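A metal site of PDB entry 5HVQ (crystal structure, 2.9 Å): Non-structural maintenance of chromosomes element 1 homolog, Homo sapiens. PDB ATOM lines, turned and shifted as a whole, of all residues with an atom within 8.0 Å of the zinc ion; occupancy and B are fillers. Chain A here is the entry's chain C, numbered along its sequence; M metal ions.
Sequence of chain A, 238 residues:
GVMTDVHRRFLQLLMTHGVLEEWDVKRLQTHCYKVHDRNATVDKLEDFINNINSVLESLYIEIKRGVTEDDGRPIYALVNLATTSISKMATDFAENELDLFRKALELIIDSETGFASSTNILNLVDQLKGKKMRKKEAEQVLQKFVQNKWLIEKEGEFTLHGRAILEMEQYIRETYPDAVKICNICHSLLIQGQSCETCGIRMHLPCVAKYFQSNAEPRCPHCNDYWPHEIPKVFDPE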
ATOM      1  N   VAL A  67       3.085 -26.264  10.083  1.00  0.00           N
ATOM      2  CA  VAL A  67       2.721 -24.927  10.551  1.00  0.00           C
ATOM      3  C   VAL A  67       3.409 -23.867   9.707  1.00  0.00           C
ATOM      4  O   VAL A  67       4.595 -23.983   9.370  1.00  0.00           O
ATOM      5  CB  VAL A  67       3.072 -24.733  12.036  1.00  0.00           C
ATOM      6  CG1 VAL A  67       2.098 -25.497  12.921  1.00  0.00           C
ATOM      7  CG2 VAL A  67       4.506 -25.165  12.319  1.00  0.00           C
ATOM      8  N   GLU A  69       5.086 -20.224   8.582  1.00  0.00           N
ATOM      9  CA  GLU A  69       6.180 -19.500   9.207  1.00  0.00           C
ATOM     10  C   GLU A  69       5.880 -18.026   9.439  1.00  0.00           C
ATOM     11  O   GLU A  69       6.727 -17.287   9.936  1.00  0.00           O
ATOM     12  CB  GLU A  69       7.453 -19.638   8.369  1.00  0.00           C
ATOM     13  CG  GLU A  69       8.051 -21.035   8.360  1.00  0.00           C
ATOM     14  CD  GLU A  69       9.390 -21.090   7.667  1.00  0.00           C
ATOM     15  OE1 GLU A  69       9.728 -20.121   6.956  1.00  0.00           O
ATOM     16  OE2 GLU A  69      10.117 -22.097   7.847  1.00  0.00           O
ATOM     17  N   ILE A 182      18.217 -23.651  10.472  1.00  0.00           N
ATOM     18  CA  ILE A 182      17.324 -24.445  11.314  1.00  0.00           C
ATOM     19  C   ILE A 182      16.894 -23.646  12.538  1.00  0.00           C
ATOM     20  O   ILE A 182      17.637 -22.802  13.049  1.00  0.00           O
ATOM     21  CB  ILE A 182      17.989 -25.774  11.758  1.00  0.00           C
ATOM     22  CG1 ILE A 182      19.145 -25.505  12.727  1.00  0.00           C
ATOM     23  CG2 ILE A 182      18.466 -26.558  10.547  1.00  0.00           C
ATOM     24  CD1 ILE A 182      19.727 -26.770  13.337  1.00  0.00           C
ATOM     25  N   CYS A 183      15.666 -23.913  12.992  1.00  0.00           N
ATOM     26  CA  CYS A 183      15.138 -23.248  14.171  1.00  0.00           C
ATOM     27  C   CYS A 183      15.778 -23.818  15.434  1.00  0.00           C
ATOM     28  O   CYS A 183      16.007 -25.024  15.526  1.00  0.00           O
ATOM     29  CB  CYS A 183      13.615 -23.405  14.233  1.00  0.00           C
ATOM     30  SG  CYS A 183      12.841 -22.698  15.708  1.00  0.00           S
ATOM     31  N   ASN A 184      16.080 -22.953  16.394  1.00  0.00           N
ATOM     32  CA  ASN A 184      16.729 -23.386  17.626  1.00  0.00           C
ATOM     33  C   ASN A 184      15.766 -24.154  18.539  1.00  0.00           C
ATOM     34  O   ASN A 184      16.196 -24.894  19.416  1.00  0.00           O
ATOM     35  CB  ASN A 184      17.299 -22.181  18.374  1.00  0.00           C
ATOM     36  CG  ASN A 184      18.098 -22.582  19.601  1.00  0.00           C
ATOM     37  OD1 ASN A 184      19.257 -22.979  19.506  1.00  0.00           O
ATOM     38  ND2 ASN A 184      17.482 -22.464  20.772  1.00  0.00           N
ATOM     39  N   ILE A 185      14.476 -23.982  18.296  1.00  0.00           N
ATOM     40  CA  ILE A 185      13.446 -24.592  19.138  1.00  0.00           C
ATOM     41  C   ILE A 185      12.974 -25.942  18.613  1.00  0.00           C
ATOM     42  O   ILE A 185      12.987 -26.941  19.343  1.00  0.00           O
ATOM     43  CB  ILE A 185      12.225 -23.664  19.292  1.00  0.00           C
ATOM     44  CG1 ILE A 185      12.653 -22.312  19.867  1.00  0.00           C
ATOM     45  CG2 ILE A 185      11.173 -24.312  20.178  1.00  0.00           C
ATOM     46  CD1 ILE A 185      13.315 -22.407  21.223  1.00  0.00           C
ATOM     47  N   CYS A 186      12.549 -25.973  17.355  1.00  0.00           N
ATOM     48  CA  CYS A 186      11.959 -27.188  16.784  1.00  0.00           C
ATOM     49  C   CYS A 186      12.944 -27.961  15.904  1.00  0.00           C
ATOM     50  O   CYS A 186      12.624 -29.052  15.421  1.00  0.00           O
ATOM     51  CB  CYS A 186      10.716 -26.833  15.966  1.00  0.00           C
ATOM     52  SG  CYS A 186      11.042 -25.881  14.472  1.00  0.00           S
ATOM     53  N   HIS A 187      14.125 -27.388  15.701  1.00  0.00           N
ATOM     54  CA  HIS A 187      15.200 -28.039  14.940  1.00  0.00           C
ATOM     55  C   HIS A 187      14.791 -28.391  13.510  1.00  0.00           C
ATOM     56  O   HIS A 187      15.336 -29.321  12.923  1.00  0.00           O
ATOM     57  CB  HIS A 187      15.684 -29.293  15.671  1.00  0.00           C
ATOM     58  CG  HIS A 187      16.073 -29.052  17.096  1.00  0.00           C
ATOM     59  ND1 HIS A 187      15.582 -29.810  18.141  1.00  0.00           N
ATOM     60  CD2 HIS A 187      16.908 -28.147  17.648  1.00  0.00           C
ATOM     61  CE1 HIS A 187      16.107 -29.379  19.269  1.00  0.00           C
ATOM     62  NE2 HIS A 187      16.907 -28.373  19.009  1.00  0.00           N
ATOM     63  N   SER A 188      13.843 -27.649  12.960  1.00  0.00           N
ATOM     64  CA  SER A 188      13.358 -27.889  11.601  1.00  0.00           C
ATOM     65  C   SER A 188      13.849 -26.811  10.642  1.00  0.00           C
ATOM     66  O   SER A 188      14.410 -25.803  11.065  1.00  0.00           O
ATOM     67  CB  SER A 188      11.836 -27.964  11.574  1.00  0.00           C
ATOM     68  OG  SER A 188      11.356 -29.010  12.392  1.00  0.00           O
ATOM     69  N   LEU A 189      13.630 -27.031   9.351  1.00  0.00           N
ATOM     70  CA  LEU A 189      14.062 -26.090   8.309  1.00  0.00           C
ATOM     71  C   LEU A 189      13.433 -24.718   8.505  1.00  0.00           C
ATOM     72  O   LEU A 189      12.242 -24.606   8.778  1.00  0.00           O
ATOM     73  CB  LEU A 189      13.726 -26.629   6.920  1.00  0.00           C
ATOM     74  CG  LEU A 189      14.003 -25.700   5.728  1.00  0.00           C
ATOM     75  CD1 LEU A 189      15.481 -25.380   5.621  1.00  0.00           C
ATOM     76  CD2 LEU A 189      13.473 -26.311   4.439  1.00  0.00           C
ATOM     77  N   LEU A 190      14.252 -23.682   8.369  1.00  0.00           N
ATOM     78  CA  LEU A 190      13.783 -22.304   8.548  1.00  0.00           C
ATOM     79  C   LEU A 190      14.061 -21.456   7.315  1.00  0.00           C
ATOM     80  O   LEU A 190      15.196 -21.364   6.848  1.00  0.00           O
ATOM     81  CB  LEU A 190      14.438 -21.681   9.775  1.00  0.00           C
ATOM     82  CG  LEU A 190      14.007 -20.272  10.187  1.00  0.00           C
ATOM     83  CD1 LEU A 190      13.980 -20.172  11.693  1.00  0.00           C
ATOM     84  CD2 LEU A 190      14.946 -19.220   9.610  1.00  0.00           C
ATOM     85  N   GLN A 192      12.078 -18.089   6.847  1.00  0.00           N
ATOM     86  CA  GLN A 192      11.992 -16.782   7.479  1.00  0.00           C
ATOM     87  C   GLN A 192      11.869 -16.936   8.990  1.00  0.00           C
ATOM     88  O   GLN A 192      11.372 -17.950   9.472  1.00  0.00           O
ATOM     89  CB  GLN A 192      10.803 -15.988   6.927  1.00  0.00           C
ATOM     90  CG  GLN A 192       9.447 -16.639   7.184  1.00  0.00           C
ATOM     91  CD  GLN A 192       8.317 -15.921   6.478  1.00  0.00           C
ATOM     92  OE1 GLN A 192       7.837 -14.885   6.943  1.00  0.00           O
ATOM     93  NE2 GLN A 192       7.880 -16.466   5.354  1.00  0.00           N
ATOM     94  N   ARG A 202      18.472 -18.800  15.175  1.00  0.00           N
ATOM     95  CA  ARG A 202      17.239 -18.312  14.556  1.00  0.00           C
ATOM     96  C   ARG A 202      16.031 -19.114  15.026  1.00  0.00           C
ATOM     97  O   ARG A 202      16.163 -20.281  15.401  1.00  0.00           O
ATOM     98  CB  ARG A 202      17.351 -18.361  13.034  1.00  0.00           C
ATOM     99  CG  ARG A 202      18.374 -17.404  12.437  1.00  0.00           C
ATOM    100  CD  ARG A 202      18.340 -17.457  10.922  1.00  0.00           C
ATOM    101  NE  ARG A 202      19.114 -16.379  10.307  1.00  0.00           N
ATOM    102  CZ  ARG A 202      20.394 -16.479   9.949  1.00  0.00           C
ATOM    103  NH1 ARG A 202      21.051 -17.619  10.149  1.00  0.00           N
ATOM    104  NH2 ARG A 202      21.016 -15.446   9.399  1.00  0.00           N
ATOM    105  N   MET A 203      14.861 -18.488  14.992  1.00  0.00           N
ATOM    106  CA  MET A 203      13.620 -19.147  15.398  1.00  0.00           C
ATOM    107  C   MET A 203      12.494 -18.872  14.420  1.00  0.00           C
ATOM    108  O   MET A 203      12.358 -17.770  13.902  1.00  0.00           O
ATOM    109  CB  MET A 203      13.185 -18.700  16.794  1.00  0.00           C
ATOM    110  CG  MET A 203      14.178 -18.979  17.901  1.00  0.00           C
ATOM    111  SD  MET A 203      13.436 -18.605  19.502  1.00  0.00           S
ATOM    112  CE  MET A 203      14.877 -18.066  20.408  1.00  0.00           C
ATOM    113  N   HIS A 204      11.669 -19.891  14.177  1.00  0.00           N
ATOM    114  CA  HIS A 204      10.413 -19.698  13.463  1.00  0.00           C
ATOM    115  C   HIS A 204       9.547 -18.743  14.268  1.00  0.00           C
ATOM    116  O   HIS A 204       9.441 -18.894  15.480  1.00  0.00           O
ATOM    117  CB  HIS A 204       9.685 -21.021  13.261  1.00  0.00           C
ATOM    118  CG  HIS A 204      10.351 -21.940  12.287  1.00  0.00           C
ATOM    119  ND1 HIS A 204      10.653 -23.253  12.592  1.00  0.00           N
ATOM    120  CD2 HIS A 204      10.771 -21.744  11.019  1.00  0.00           C
ATOM    121  CE1 HIS A 204      11.227 -23.818  11.544  1.00  0.00           C
ATOM    122  NE2 HIS A 204      11.315 -22.926  10.577  1.00  0.00           N
ATOM    123  N   LEU A 205       8.930 -17.783  13.596  1.00  0.00           N
ATOM    124  CA  LEU A 205       8.020 -16.835  14.251  1.00  0.00           C
ATOM    125  C   LEU A 205       6.992 -17.504  15.193  1.00  0.00           C
ATOM    126  O   LEU A 205       6.764 -16.999  16.287  1.00  0.00           O
ATOM    127  CB  LEU A 205       7.281 -15.999  13.200  1.00  0.00           C
ATOM    128  CG  LEU A 205       7.796 -14.575  12.977  1.00  0.00           C
ATOM    129  CD1 LEU A 205       9.275 -14.582  12.630  1.00  0.00           C
ATOM    130  CD2 LEU A 205       6.990 -13.875  11.886  1.00  0.00           C
ATOM    131  N   PRO A 206       6.385 -18.636  14.778  1.00  0.00           N
ATOM    132  CA  PRO A 206       5.477 -19.284  15.741  1.00  0.00           C
ATOM    133  C   PRO A 206       6.207 -19.936  16.909  1.00  0.00           C
ATOM    134  O   PRO A 206       5.603 -20.167  17.952  1.00  0.00           O
ATOM    135  CB  PRO A 206       4.780 -20.351  14.891  1.00  0.00           C
ATOM    136  CG  PRO A 206       4.984 -19.933  13.483  1.00  0.00           C
ATOM    137  CD  PRO A 206       6.307 -19.271  13.451  1.00  0.00           C
ATOM    138  N   CYS A 207       7.496 -20.220  16.742  1.00  0.00           N
ATOM    139  CA  CYS A 207       8.272 -20.862  17.799  1.00  0.00           C
ATOM    140  C   CYS A 207       8.673 -19.873  18.883  1.00  0.00           C
ATOM    141  O   CYS A 207       8.647 -20.204  20.069  1.00  0.00           O
ATOM    142  CB  CYS A 207       9.517 -21.532  17.218  1.00  0.00           C
ATOM    143  SG  CYS A 207       9.154 -22.993  16.206  1.00  0.00           S
ATOM    144  N   VAL A 208       9.034 -18.656  18.496  1.00  0.00           N
ATOM    145  CA  VAL A 208       9.342 -17.616  19.465  1.00  0.00           C
ATOM    146  C   VAL A 208       8.043 -17.202  20.162  1.00  0.00           C
ATOM    147  O   VAL A 208       8.057 -16.773  21.318  1.00  0.00           O
ATOM    148  CB  VAL A 208      10.025 -16.376  18.808  1.00  0.00           C
ATOM    149  CG1 VAL A 208      10.296 -16.618  17.340  1.00  0.00           C
ATOM    150  CG2 VAL A 208       9.202 -15.104  18.987  1.00  0.00           C
HETATM  151 ZN    ZN M   1      10.882 -23.628  14.847  1.00  0.00          ZN
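The backbone carbonyl oxygen (O) of Cys 186 sits at hydrogen-bond distance from the side-chain hydroxyl (OG) of Ser 188 (3.3 Å).
A ring nitrogen (NE2) of His 204 lies within hydrogen-bond range of the backbone carbonyl oxygen of Leu 189.
NE2 of His 204 lies within hydrogen-bond range of OE2 of Glu 69.
SG of Cys 183 lies close to N of Ile 185, 3.3 Å away.
The backbone NH (N) of Cys 183 sits at hydrogen-bond distance from the backbone carbonyl oxygen (O) of Ser 188, at 3.0 Å.
Four residues have an atom within 4 Å of the zinc ion: Cys 183, Cys 186, His 204 and Cys 207.
The zinc ion is bound by SG of Cys 207, at 2.3 Å.
SG of Cys 186 is bound to the zinc ion, at 2.3 Å.
A ring nitrogen (ND1) of His 204 binds the zinc ion (2.3 Å).
The side-chain sulfur (SG) of Cys 183 binds the zinc ion.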
